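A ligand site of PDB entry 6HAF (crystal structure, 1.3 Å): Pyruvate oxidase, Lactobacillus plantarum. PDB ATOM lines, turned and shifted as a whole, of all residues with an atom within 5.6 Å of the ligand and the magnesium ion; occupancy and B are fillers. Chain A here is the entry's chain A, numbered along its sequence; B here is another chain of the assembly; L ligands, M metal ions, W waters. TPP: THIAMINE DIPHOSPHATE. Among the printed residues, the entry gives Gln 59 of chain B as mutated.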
ATOM      1  N   ASN A  92       6.629   7.643 -19.501  1.00  0.00           N
ATOM      2  CA  ASN A  92       7.689   7.027 -18.687  1.00  0.00           C
ATOM      3  C   ASN A  92       8.004   7.843 -17.435  1.00  0.00           C
ATOM      4  O   ASN A  92       8.305   7.271 -16.366  1.00  0.00           O
ATOM      5  CB  ASN A  92       8.924   6.709 -19.478  1.00  0.00           C
ATOM      6  CG  ASN A  92       8.774   5.426 -20.257  1.00  0.00           C
ATOM      7  OD1 ASN A  92       7.756   5.223 -20.919  1.00  0.00           O
ATOM      8  ND2 ASN A  92       9.748   4.521 -20.129  1.00  0.00           N
ATOM      9  N   ASP A 393      21.219   6.880 -14.066  1.00  0.00           N
ATOM     10  CA  ASP A 393      20.339   6.200 -15.007  1.00  0.00           C
ATOM     11  C   ASP A 393      20.152   4.747 -14.521  1.00  0.00           C
ATOM     12  O   ASP A 393      20.337   4.476 -13.319  1.00  0.00           O
ATOM     13  CB  ASP A 393      20.905   6.322 -16.430  1.00  0.00           C
ATOM     14  CG  ASP A 393      19.834   6.379 -17.489  1.00  0.00           C
ATOM     15  OD1 ASP A 393      19.254   5.320 -17.800  1.00  0.00           O
ATOM     16  OD2 ASP A 393      19.605   7.484 -18.040  1.00  0.00           O
ATOM     17  N   VAL A 394      19.757   3.839 -15.430  1.00  0.00           N
ATOM     18  CA  VAL A 394      19.338   2.492 -15.038  1.00  0.00           C
ATOM     19  C   VAL A 394      20.153   1.455 -15.791  1.00  0.00           C
ATOM     20  O   VAL A 394      20.192   1.456 -17.023  1.00  0.00           O
ATOM     21  CB  VAL A 394      17.835   2.300 -15.325  1.00  0.00           C
ATOM     22  CG1 VAL A 394      17.370   0.856 -15.159  1.00  0.00           C
ATOM     23  CG2 VAL A 394      17.009   3.205 -14.400  1.00  0.00           C
ATOM     24  N   GLY A 395      20.737   0.540 -15.036  1.00  0.00           N
ATOM     25  CA  GLY A 395      21.562  -0.523 -15.587  1.00  0.00           C
ATOM     26  C   GLY A 395      22.731  -0.853 -14.683  1.00  0.00           C
ATOM     27  O   GLY A 395      22.642  -0.663 -13.469  1.00  0.00           O
ATOM     28  N   ASP A 396      23.844  -1.300 -15.264  1.00  0.00           N
ATOM     29  CA  ASP A 396      25.033  -1.574 -14.432  1.00  0.00           C
ATOM     30  C   ASP A 396      25.436  -0.363 -13.589  1.00  0.00           C
ATOM     31  O   ASP A 396      26.024  -0.531 -12.534  1.00  0.00           O
ATOM     32  CB  ASP A 396      26.250  -1.969 -15.276  1.00  0.00           C
ATOM     33  CG  ASP A 396      26.279  -3.423 -15.720  1.00  0.00           C
ATOM     34  OD1 ASP A 396      25.523  -4.269 -15.187  1.00  0.00           O
ATOM     35  OD2 ASP A 396      27.091  -3.715 -16.647  1.00  0.00           O
ATOM     36  N   ILE A 397      25.114   0.845 -14.032  1.00  0.00           N
ATOM     37  CA  ILE A 397      25.526   2.006 -13.265  1.00  0.00           C
ATOM     38  C   ILE A 397      24.897   2.024 -11.882  1.00  0.00           C
ATOM     39  O   ILE A 397      25.505   2.530 -10.947  1.00  0.00           O
ATOM     40  CB  ILE A 397      25.246   3.347 -14.001  1.00  0.00           C
ATOM     41  CG1 ILE A 397      25.868   4.540 -13.274  1.00  0.00           C
ATOM     42  CG2 ILE A 397      23.710   3.595 -14.225  1.00  0.00           C
ATOM     43  CD1 ILE A 397      27.346   4.515 -13.092  1.00  0.00           C
ATOM     44  N   PHE A 419       9.919   1.833 -10.907  1.00  0.00           N
ATOM     45  CA  PHE A 419       9.581   1.678 -12.314  1.00  0.00           C
ATOM     46  C   PHE A 419      10.841   1.436 -13.119  1.00  0.00           C
ATOM     47  O   PHE A 419      10.819   0.765 -14.137  1.00  0.00           O
ATOM     48  CB  PHE A 419       8.864   2.946 -12.794  1.00  0.00           C
ATOM     49  CG  PHE A 419       8.235   2.840 -14.152  1.00  0.00           C
ATOM     50  CD1 PHE A 419       7.224   1.914 -14.386  1.00  0.00           C
ATOM     51  CD2 PHE A 419       8.609   3.676 -15.171  1.00  0.00           C
ATOM     52  CE1 PHE A 419       6.609   1.837 -15.602  1.00  0.00           C
ATOM     53  CE2 PHE A 419       7.961   3.620 -16.425  1.00  0.00           C
ATOM     54  CZ  PHE A 419       6.991   2.670 -16.632  1.00  0.00           C
ATOM     55  N   ALA A 420      11.961   1.977 -12.652  1.00  0.00           N
ATOM     56  CA  ALA A 420      13.294   1.767 -13.246  1.00  0.00           C
ATOM     57  C   ALA A 420      13.316   2.056 -14.734  1.00  0.00           C
ATOM     58  O   ALA A 420      13.846   1.287 -15.523  1.00  0.00           O
ATOM     59  CB  ALA A 420      13.817   0.357 -12.949  1.00  0.00           C
ATOM     60  N   THR A 421      12.800   3.223 -15.106  1.00  0.00           N
ATOM     61  CA  THR A 421      12.919   3.651 -16.486  1.00  0.00           C
ATOM     62  C   THR A 421      14.327   4.156 -16.828  1.00  0.00           C
ATOM     63  O   THR A 421      14.850   5.099 -16.248  1.00  0.00           O
ATOM     64  CB  THR A 421      11.856   4.693 -16.921  1.00  0.00           C
ATOM     65  OG1 THR A 421      12.044   4.983 -18.302  1.00  0.00           O
ATOM     66  CG2 THR A 421      11.909   5.968 -16.109  1.00  0.00           C
ATOM     67  N   MET A 422      14.934   3.543 -17.831  1.00  0.00           N
ATOM     68  CA  MET A 422      16.138   4.074 -18.438  1.00  0.00           C
ATOM     69  C   MET A 422      15.828   5.473 -18.972  1.00  0.00           C
ATOM     70  O   MET A 422      14.676   5.810 -19.291  1.00  0.00           O
ATOM     71  CB  MET A 422      16.592   3.179 -19.582  1.00  0.00           C
ATOM     72  CG  MET A 422      17.212   1.873 -19.149  1.00  0.00           C
ATOM     73  SD  MET A 422      17.350   0.732 -20.531  1.00  0.00           S
ATOM     74  CE  MET A 422      18.561   1.552 -21.528  1.00  0.00           C
ATOM     75  N   ALA A 445      25.387   7.641 -16.463  1.00  0.00           N
ATOM     76  CA  ALA A 445      24.479   6.903 -17.327  1.00  0.00           C
ATOM     77  C   ALA A 445      25.224   5.872 -18.165  1.00  0.00           C
ATOM     78  O   ALA A 445      26.300   6.159 -18.676  1.00  0.00           O
ATOM     79  CB  ALA A 445      23.704   7.858 -18.244  1.00  0.00           C
ATOM     80  N   GLY A 446      24.601   4.717 -18.381  1.00  0.00           N
ATOM     81  CA  GLY A 446      25.088   3.814 -19.393  1.00  0.00           C
ATOM     82  C   GLY A 446      24.780   4.332 -20.778  1.00  0.00           C
ATOM     83  O   GLY A 446      23.958   5.227 -20.957  1.00  0.00           O
ATOM     84  N   ASP A 447      25.443   3.755 -21.779  1.00  0.00           N
ATOM     85  CA  ASP A 447      25.234   4.163 -23.153  1.00  0.00           C
ATOM     86  C   ASP A 447      23.809   3.902 -23.640  1.00  0.00           C
ATOM     87  O   ASP A 447      23.254   4.699 -24.392  1.00  0.00           O
ATOM     88  CB  ASP A 447      26.293   3.600 -24.112  1.00  0.00           C
ATOM     89  CG  ASP A 447      26.546   2.082 -24.017  1.00  0.00           C
ATOM     90  OD1 ASP A 447      25.968   1.331 -23.182  1.00  0.00           O
ATOM     91  OD2 ASP A 447      27.415   1.670 -24.815  1.00  0.00           O
ATOM     92  N   GLY A 448      23.191   2.804 -23.229  1.00  0.00           N
ATOM     93  CA  GLY A 448      21.833   2.508 -23.632  1.00  0.00           C
ATOM     94  C   GLY A 448      20.868   3.550 -23.085  1.00  0.00           C
ATOM     95  O   GLY A 448      20.017   4.086 -23.809  1.00  0.00           O
ATOM     96  N   GLY A 449      21.030   3.893 -21.820  1.00  0.00           N
ATOM     97  CA  GLY A 449      20.149   4.859 -21.182  1.00  0.00           C
ATOM     98  C   GLY A 449      20.357   6.281 -21.672  1.00  0.00           C
ATOM     99  O   GLY A 449      19.408   7.030 -21.923  1.00  0.00           O
ATOM    100  N   ALA A 450      21.613   6.679 -21.804  1.00  0.00           N
ATOM    101  CA  ALA A 450      21.953   7.990 -22.311  1.00  0.00           C
ATOM    102  C   ALA A 450      21.424   8.128 -23.724  1.00  0.00           C
ATOM    103  O   ALA A 450      20.933   9.207 -24.105  1.00  0.00           O
ATOM    104  CB  ALA A 450      23.476   8.183 -22.286  1.00  0.00           C
ATOM    105  N   MET A 452      18.758   6.915 -24.989  1.00  0.00           N
ATOM    106  CA  MET A 452      17.318   7.096 -25.028  1.00  0.00           C
ATOM    107  C   MET A 452      16.889   8.550 -24.908  1.00  0.00           C
ATOM    108  O   MET A 452      15.861   8.931 -25.445  1.00  0.00           O
ATOM    109  CB  MET A 452      16.613   6.248 -23.971  1.00  0.00           C
ATOM    110  CG  MET A 452      16.591   4.788 -24.378  1.00  0.00           C
ATOM    111  SD  MET A 452      15.787   3.796 -23.127  1.00  0.00           S
ATOM    112  CE  MET A 452      15.880   2.203 -23.894  1.00  0.00           C
ATOM    113  N   PHE A 472      28.889   5.677 -19.713  1.00  0.00           N
ATOM    114  CA  PHE A 472      29.664   4.423 -19.588  1.00  0.00           C
ATOM    115  C   PHE A 472      29.388   3.588 -20.842  1.00  0.00           C
ATOM    116  O   PHE A 472      28.358   2.938 -20.948  1.00  0.00           O
ATOM    117  CB  PHE A 472      29.232   3.701 -18.305  1.00  0.00           C
ATOM    118  CG  PHE A 472      29.658   4.385 -17.026  1.00  0.00           C
ATOM    119  CD1 PHE A 472      30.665   3.827 -16.239  1.00  0.00           C
ATOM    120  CD2 PHE A 472      29.085   5.553 -16.604  1.00  0.00           C
ATOM    121  CE1 PHE A 472      31.052   4.462 -15.070  1.00  0.00           C
ATOM    122  CE2 PHE A 472      29.482   6.165 -15.457  1.00  0.00           C
ATOM    123  CZ  PHE A 472      30.462   5.626 -14.695  1.00  0.00           C
ATOM    124  N   THR A 473      30.309   3.673 -21.802  1.00  0.00           N
ATOM    125  CA  THR A 473      30.124   3.096 -23.121  1.00  0.00           C
ATOM    126  C   THR A 473      30.766   1.718 -23.149  1.00  0.00           C
ATOM    127  O   THR A 473      31.982   1.595 -23.257  1.00  0.00           O
ATOM    128  CB  THR A 473      30.614   4.030 -24.220  1.00  0.00           C
ATOM    129  OG1 THR A 473      29.716   5.157 -24.280  1.00  0.00           O
ATOM    130  CG2 THR A 473      30.615   3.317 -25.582  1.00  0.00           C
ATOM    131  N   ASN A 474      29.918   0.683 -23.007  1.00  0.00           N
ATOM    132  CA  ASN A 474      30.328  -0.691 -23.191  1.00  0.00           C
ATOM    133  C   ASN A 474      29.824  -1.319 -24.479  1.00  0.00           C
ATOM    134  O   ASN A 474      30.129  -2.462 -24.732  1.00  0.00           O
ATOM    135  CB  ASN A 474      29.945  -1.573 -21.979  1.00  0.00           C
ATOM    136  CG  ASN A 474      28.495  -1.427 -21.563  1.00  0.00           C
ATOM    137  OD1 ASN A 474      27.671  -0.939 -22.317  1.00  0.00           O
ATOM    138  ND2 ASN A 474      28.181  -1.858 -20.362  1.00  0.00           N
ATOM    139  N   CYS A 475      29.061  -0.562 -25.277  1.00  0.00           N
ATOM    140  CA  CYS A 475      28.416  -1.085 -26.490  1.00  0.00           C
ATOM    141  C   CYS A 475      27.534  -2.274 -26.168  1.00  0.00           C
ATOM    142  O   CYS A 475      27.397  -3.199 -26.979  1.00  0.00           O
ATOM    143  CB  CYS A 475      29.435  -1.448 -27.579  1.00  0.00           C
ATOM    144  SG  CYS A 475      30.351  -0.001 -28.166  1.00  0.00           S
ATOM    145  N   GLN A 476      26.898  -2.225 -25.003  1.00  0.00           N
ATOM    146  CA  GLN A 476      26.035  -3.295 -24.533  1.00  0.00           C
ATOM    147  C   GLN A 476      24.892  -2.767 -23.703  1.00  0.00           C
ATOM    148  O   GLN A 476      24.980  -1.699 -23.091  1.00  0.00           O
ATOM    149  CB  GLN A 476      26.789  -4.275 -23.632  1.00  0.00           C
ATOM    150  CG  GLN A 476      27.954  -4.948 -24.245  1.00  0.00           C
ATOM    151  CD  GLN A 476      28.746  -5.762 -23.224  1.00  0.00           C
ATOM    152  OE1 GLN A 476      28.696  -5.500 -22.022  1.00  0.00           O
ATOM    153  NE2 GLN A 476      29.489  -6.720 -23.694  1.00  0.00           N
ATOM    154  N   TYR A 477      23.828  -3.548 -23.635  1.00  0.00           N
ATOM    155  CA  TYR A 477      22.899  -3.456 -22.520  1.00  0.00           C
ATOM    156  C   TYR A 477      23.478  -4.444 -21.500  1.00  0.00           C
ATOM    157  O   TYR A 477      23.046  -5.605 -21.411  1.00  0.00           O
ATOM    158  CB  TYR A 477      21.490  -3.868 -22.925  1.00  0.00           C
ATOM    159  CG  TYR A 477      20.816  -2.932 -23.917  1.00  0.00           C
ATOM    160  CD1 TYR A 477      20.730  -1.569 -23.663  1.00  0.00           C
ATOM    161  CD2 TYR A 477      20.272  -3.418 -25.070  1.00  0.00           C
ATOM    162  CE1 TYR A 477      20.116  -0.721 -24.579  1.00  0.00           C
ATOM    163  CE2 TYR A 477      19.658  -2.587 -25.971  1.00  0.00           C
ATOM    164  CZ  TYR A 477      19.576  -1.237 -25.720  1.00  0.00           C
ATOM    165  OH  TYR A 477      18.976  -0.437 -26.638  1.00  0.00           O
ATOM    166  N   GLY A 478      24.509  -4.010 -20.780  1.00  0.00           N
ATOM    167  CA  GLY A 478      25.287  -4.948 -19.955  1.00  0.00           C
ATOM    168  C   GLY A 478      24.472  -5.675 -18.903  1.00  0.00           C
ATOM    169  O   GLY A 478      24.579  -6.908 -18.709  1.00  0.00           O
ATOM    170  N   PHE A 479      23.619  -4.904 -18.216  1.00  0.00           N
ATOM    171  CA  PHE A 479      22.787  -5.473 -17.160  1.00  0.00           C
ATOM    172  C   PHE A 479      21.953  -6.646 -17.695  1.00  0.00           C
ATOM    173  O   PHE A 479      21.728  -7.636 -16.997  1.00  0.00           O
ATOM    174  CB  PHE A 479      21.877  -4.359 -16.638  1.00  0.00           C
ATOM    175  CG  PHE A 479      21.423  -4.505 -15.211  1.00  0.00           C
ATOM    176  CD1 PHE A 479      22.311  -4.370 -14.168  1.00  0.00           C
ATOM    177  CD2 PHE A 479      20.087  -4.691 -14.929  1.00  0.00           C
ATOM    178  CE1 PHE A 479      21.876  -4.457 -12.867  1.00  0.00           C
ATOM    179  CE2 PHE A 479      19.650  -4.759 -13.619  1.00  0.00           C
ATOM    180  CZ  PHE A 479      20.554  -4.641 -12.576  1.00  0.00           C
ATOM    181  N   ILE A 480      21.470  -6.500 -18.927  1.00  0.00           N
ATOM    182  CA  ILE A 480      20.641  -7.535 -19.562  1.00  0.00           C
ATOM    183  C   ILE A 480      21.480  -8.667 -20.163  1.00  0.00           C
ATOM    184  O   ILE A 480      21.044  -9.829 -20.112  1.00  0.00           O
ATOM    185  CB  ILE A 480      19.736  -6.944 -20.659  1.00  0.00           C
ATOM    186  CG1 ILE A 480      18.986  -5.741 -20.114  1.00  0.00           C
ATOM    187  CG2 ILE A 480      18.769  -7.995 -21.199  1.00  0.00           C
ATOM    188  CD1 ILE A 480      18.216  -5.968 -18.812  1.00  0.00           C
ATOM    189  N   PHE A 497      25.740  -4.075 -29.276  1.00  0.00           N
ATOM    190  CA  PHE A 497      25.344  -3.192 -30.351  1.00  0.00           C
ATOM    191  C   PHE A 497      26.483  -2.269 -30.763  1.00  0.00           C
ATOM    192  O   PHE A 497      27.572  -2.326 -30.197  1.00  0.00           O
ATOM    193  CB  PHE A 497      24.074  -2.410 -29.994  1.00  0.00           C
ATOM    194  CG  PHE A 497      24.087  -1.751 -28.642  1.00  0.00           C
ATOM    195  CD1 PHE A 497      24.939  -0.691 -28.354  1.00  0.00           C
ATOM    196  CD2 PHE A 497      23.198  -2.173 -27.660  1.00  0.00           C
ATOM    197  CE1 PHE A 497      24.915  -0.086 -27.083  1.00  0.00           C
ATOM    198  CE2 PHE A 497      23.171  -1.570 -26.426  1.00  0.00           C
ATOM    199  CZ  PHE A 497      24.022  -0.539 -26.139  1.00  0.00           C
ATOM    200  N   ILE B  32      13.659  -4.113 -27.605  1.00  0.00           N
ATOM    201  CA  ILE B  32      14.837  -4.004 -26.733  1.00  0.00           C
ATOM    202  C   ILE B  32      14.592  -5.074 -25.671  1.00  0.00           C
ATOM    203  O   ILE B  32      13.501  -5.152 -25.108  1.00  0.00           O
ATOM    204  CB  ILE B  32      14.944  -2.595 -26.127  1.00  0.00           C
ATOM    205  CG1 ILE B  32      15.273  -1.579 -27.221  1.00  0.00           C
ATOM    206  CG2 ILE B  32      15.946  -2.561 -24.939  1.00  0.00           C
ATOM    207  CD1 ILE B  32      15.323  -0.174 -26.760  1.00  0.00           C
ATOM    208  N   PRO B  33      15.607  -5.903 -25.377  1.00  0.00           N
ATOM    209  CA  PRO B  33      15.426  -6.993 -24.397  1.00  0.00           C
ATOM    210  C   PRO B  33      15.441  -6.464 -22.979  1.00  0.00           C
ATOM    211  O   PRO B  33      15.809  -5.325 -22.680  1.00  0.00           O
ATOM    212  CB  PRO B  33      16.654  -7.864 -24.650  1.00  0.00           C
ATOM    213  CG  PRO B  33      17.707  -6.861 -25.012  1.00  0.00           C
ATOM    214  CD  PRO B  33      16.981  -5.867 -25.916  1.00  0.00           C
ATOM    215  N   GLY B  34      14.964  -7.324 -22.095  1.00  0.00           N
ATOM    216  CA  GLY B  34      15.021  -7.124 -20.650  1.00  0.00           C
ATOM    217  C   GLY B  34      14.768  -8.461 -20.004  1.00  0.00           C
ATOM    218  O   GLY B  34      14.272  -9.386 -20.641  1.00  0.00           O
ATOM    219  N   GLN B  59      12.241   2.083 -27.620  1.00  0.00           N
ATOM    220  CA  GLN B  59      11.122   1.259 -28.040  1.00  0.00           C
ATOM    221  C   GLN B  59      10.044   1.992 -28.830  1.00  0.00           C
ATOM    222  O   GLN B  59       9.294   1.332 -29.571  1.00  0.00           O
ATOM    223  CB  GLN B  59      10.472   0.542 -26.849  1.00  0.00           C
ATOM    224  CG  GLN B  59      11.410  -0.355 -26.012  1.00  0.00           C
ATOM    225  CD  GLN B  59      12.139   0.365 -24.905  1.00  0.00           C
ATOM    226  OE1 GLN B  59      12.254   1.599 -24.907  1.00  0.00           O
ATOM    227  NE2 GLN B  59      12.733  -0.393 -24.020  1.00  0.00           N
ATOM    228  N   SER B  82      10.039  -4.651 -22.876  1.00  0.00           N
ATOM    229  CA  SER B  82      10.093  -5.243 -21.566  1.00  0.00           C
ATOM    230  C   SER B  82       9.087  -4.598 -20.577  1.00  0.00           C
ATOM    231  O   SER B  82       8.471  -3.564 -20.855  1.00  0.00           O
ATOM    232  CB  SER B  82      11.546  -5.167 -21.051  1.00  0.00           C
ATOM    233  OG  SER B  82      12.023  -3.811 -21.005  1.00  0.00           O
ATOM    234  N   PRO B  85       8.615   0.224 -18.094  1.00  0.00           N
ATOM    235  CA  PRO B  85       9.078   1.287 -19.010  1.00  0.00           C
ATOM    236  C   PRO B  85       9.388   0.860 -20.435  1.00  0.00           C
ATOM    237  O   PRO B  85       9.325   1.698 -21.361  1.00  0.00           O
ATOM    238  CB  PRO B  85      10.350   1.805 -18.324  1.00  0.00           C
ATOM    239  CG  PRO B  85      10.852   0.628 -17.516  1.00  0.00           C
ATOM    240  CD  PRO B  85       9.559   0.048 -16.974  1.00  0.00           C
ATOM    241  N   GLY B  86       9.689  -0.419 -20.642  1.00  0.00           N
ATOM    242  CA  GLY B  86       9.922  -0.872 -21.998  1.00  0.00           C
ATOM    243  C   GLY B  86       8.668  -0.778 -22.831  1.00  0.00           C
ATOM    244  O   GLY B  86       8.686  -0.283 -23.956  1.00  0.00           O
ATOM    245  N   HIS B  89       7.174   2.897 -23.294  1.00  0.00           N
ATOM    246  CA  HIS B  89       7.823   3.571 -24.411  1.00  0.00           C
ATOM    247  C   HIS B  89       7.230   3.298 -25.820  1.00  0.00           C
ATOM    248  O   HIS B  89       7.451   4.068 -26.741  1.00  0.00           O
ATOM    249  CB  HIS B  89       9.297   3.228 -24.451  1.00  0.00           C
ATOM    250  CG  HIS B  89      10.201   4.201 -23.738  1.00  0.00           C
ATOM    251  ND1 HIS B  89      11.556   3.975 -23.611  1.00  0.00           N
ATOM    252  CD2 HIS B  89       9.991   5.446 -23.217  1.00  0.00           C
ATOM    253  CE1 HIS B  89      12.133   5.015 -23.039  1.00  0.00           C
ATOM    254  NE2 HIS B  89      11.208   5.922 -22.788  1.00  0.00           N
ATOM    255  N   GLN B 122       9.738  -3.528 -10.523  1.00  0.00           N
ATOM    256  CA  GLN B 122       9.163  -3.161 -11.830  1.00  0.00           C
ATOM    257  C   GLN B 122       7.973  -4.026 -12.207  1.00  0.00           C
ATOM    258  O   GLN B 122       7.689  -4.213 -13.363  1.00  0.00           O
ATOM    259  CB  GLN B 122      10.238  -3.292 -12.894  1.00  0.00           C
ATOM    260  CG  GLN B 122       9.984  -2.557 -14.217  1.00  0.00           C
ATOM    261  CD  GLN B 122      11.193  -2.661 -15.036  1.00  0.00           C
ATOM    262  OE1 GLN B 122      11.915  -1.692 -15.238  1.00  0.00           O
ATOM    263  NE2 GLN B 122      11.440  -3.849 -15.529  1.00  0.00           N
HETATM  264  N1' TPP L   1      13.789   0.010 -21.420  1.00  0.00           N
HETATM  265  C2' TPP L   1      13.609   0.990 -20.509  1.00  0.00           C
HETATM  266  CM2 TPP L   1      13.072   2.327 -20.989  1.00  0.00           C
HETATM  267  N3' TPP L   1      13.893   0.809 -19.211  1.00  0.00           N
HETATM  268  C4' TPP L   1      14.369  -0.380 -18.816  1.00  0.00           C
HETATM  269  N4' TPP L   1      14.575  -0.517 -17.505  1.00  0.00           N
HETATM  270  C5' TPP L   1      14.603  -1.409 -19.746  1.00  0.00           C
HETATM  271  C6' TPP L   1      14.303  -1.151 -21.077  1.00  0.00           C
HETATM  272  C7' TPP L   1      15.186  -2.784 -19.356  1.00  0.00           C
HETATM  273  N3  TPP L   1      16.613  -2.635 -18.986  1.00  0.00           N
HETATM  274  C2  TPP L   1      16.986  -2.511 -17.688  1.00  0.00           C
HETATM  275  S1  TPP L   1      18.726  -2.346 -17.565  1.00  0.00           S
HETATM  276  C5  TPP L   1      18.873  -2.351 -19.297  1.00  0.00           C
HETATM  277  C4  TPP L   1      17.623  -2.553 -19.892  1.00  0.00           C
HETATM  278  CM4 TPP L   1      17.401  -2.636 -21.397  1.00  0.00           C
HETATM  279  C6  TPP L   1      20.232  -2.180 -19.904  1.00  0.00           C
HETATM  280  C7  TPP L   1      20.781  -0.757 -19.676  1.00  0.00           C
HETATM  281  O7  TPP L   1      21.857  -0.643 -20.615  1.00  0.00           O
HETATM  282  PA  TPP L   1      22.892   0.563 -20.454  1.00  0.00           P
HETATM  283  O1A TPP L   1      23.805   0.514 -21.629  1.00  0.00           O
HETATM  284  O2A TPP L   1      22.163   1.850 -20.212  1.00  0.00           O
HETATM  285  O3A TPP L   1      23.697   0.178 -19.123  1.00  0.00           O
HETATM  286  PB  TPP L   1      24.824  -0.976 -18.877  1.00  0.00           P
HETATM  287  O1B TPP L   1      25.307  -1.462 -20.226  1.00  0.00           O
HETATM  288  O2B TPP L   1      24.124  -2.082 -18.026  1.00  0.00           O
HETATM  289  O3B TPP L   1      25.929  -0.193 -18.101  1.00  0.00           O
HETATM  290 MG    MG M   1      25.680  -0.186 -21.897  1.00  0.00          MG
HETATM  291  O   HOH W   1      28.409   0.241 -17.139  1.00  0.00           O
HETATM  292  O   HOH W   2      14.649  -2.773 -15.566  1.00  0.00           O
HETATM  293  O   HOH W   3      26.610   1.027 -20.437  1.00  0.00           O
HETATM  294  O   HOH W   4      11.828  -3.093 -18.537  1.00  0.00           O
HETATM  295  O   HOH W   5      24.496   1.714 -16.668  1.00  0.00           O
HETATM  296  O   HOH W   6      22.279   3.180 -17.891  1.00  0.00           O
HETATM  297  O   HOH W   7      16.865  -3.482 -14.501  1.00  0.00           O
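The magnesium ion is bound by the side-chain carboxylate (OD1) of Asp 447 (2.0 Å), an oxygen (O1A) of the ligand (2.0 Å), the backbone carbonyl oxygen (O) of Gln 476 (2.1 Å), water W3 (2.1 Å), an oxygen (O1B) of the ligand (2.1 Å) and the side-chain amide oxygen (OD1) of Asn 474 (2.2 Å).
Water W3 lies within hydrogen-bond range of O of Phe 472 (2.6 Å), O3B of the ligand (2.7 Å), N of Asp 447 (3.3 Å) and ND2 of Asn 474 (3.3 Å).
Water W6 lies within hydrogen-bond range of O2A of the ligand (2.7 Å), N of Gly 446 (2.8 Å) and O of Val 394 (2.8 Å).
Water W2 bridges OE1 of Gln 122 of chain B (3.0 Å) and N4' of the ligand (3.0 Å).
Water W4 lies within hydrogen-bond range of the side-chain hydroxyl of Ser 82 of chain B (2.6 Å) and the side-chain amide nitrogen of Gln 122 of chain B (3.1 Å).
N of Gly 478 lies within hydrogen-bond range of O2B of the ligand (3.4 Å).
O of Ala 420 lies within hydrogen-bond range of N4' of the ligand.
NE2 of Gln 59 of chain B lies within hydrogen-bond range of N1' of the ligand, at 2.8 Å.
The backbone NH (N) of Gly 449 sits at hydrogen-bond distance from an oxygen (O2A) of the ligand.
N of Gly 448 lies within hydrogen-bond range of O2A of the ligand (3.3 Å).
N of Phe 479 sits at hydrogen-bond distance from O2B of the ligand (2.9 Å).
The backbone NH of Asp 396 sits at hydrogen-bond distance from an oxygen (O2B) of the ligand (2.9 Å).
A nitrogen (N3') of the ligand is in hydrogen-bond range of the backbone NH (N) of Met 422, at 3.2 Å.
The nearest printed residue that does not touch the magnesium ion is Gly 448 (4.1 Å).
The backbone NH (N) of Asp 447 lies within hydrogen-bond range of the backbone carbonyl oxygen (O) of Phe 472 (3.1 Å).
The side-chain carboxylate (OD2) of Asp 447 sits at hydrogen-bond distance from the backbone NH (N) of Cys 475.
The side-chain amide oxygen of Gln 59 of chain B lies within hydrogen-bond range of a ring nitrogen (ND1) of His 89 of chain B (2.8 Å).
The side-chain amide nitrogen (ND2) of Asn 92 sits close to a ring nitrogen (NE2) of His 89 of chain B (3.3 Å).
The side-chain amide nitrogen of Asn 92 lies within hydrogen-bond range of the backbone carbonyl oxygen of Pro 85 of chain B (3.1 Å).
The backbone carbonyl oxygen (O) of Phe 419 lies close to the side-chain amide oxygen (OE1) of Gln 122 of chain B (2.9 Å).
ND2 of Asn 92 is in hydrogen-bond range of OG1 of Thr 421 (3.0 Å).
Val 394 touches the ligand (O to C7, 3.5 Å).
Gly 395 touches the ligand.
Thr 421 touches the ligand.
Gly 446 touches the ligand (CA to O2A, 3.6 Å).
Met 452 touches the ligand.
Tyr 477 touches the ligand (CD1 to O7, 3.4 Å).
Ile 480 touches the ligand.
Ile 32 of chain B touches the ligand (CG2 to CM4, 3.8 Å).
Pro 33 of chain B touches the ligand.
Ser 82 of chain B touches the ligand (OG to C6', 3.5 Å).
Pro 85 of chain B touches the ligand.
His 89 of chain B touches the ligand.
Gln 122 of chain B touches the ligand (OE1 to N4', 3.7 Å).
Hydrophobic or aromatic side chains that line the ligand: Val 394, Met 422, Met 452, Tyr 477, Phe 479, Ile 480, Ile 32 of chain B, Pro 85 of chain B and His 89 of chain B.
Within 4 Å of the ligand: Val 394, Gly 395, Asp 396, Ala 420, Thr 421, Met 422, Gly 446, Asp 447, Gly 448, Gly 449, Met 452, Asn 474, Gln 476, Tyr 477, Gly 478, Phe 479, Ile 480, Ile 32 of chain B, Pro 33 of chain B, Gln 59 of chain B, Ser 82 of chain B, Pro 85 of chain B, His 89 of chain B and Gln 122 of chain B.
The nearest printed residue that does not touch the ligand is Gly 86 of chain B (4.01 Å).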
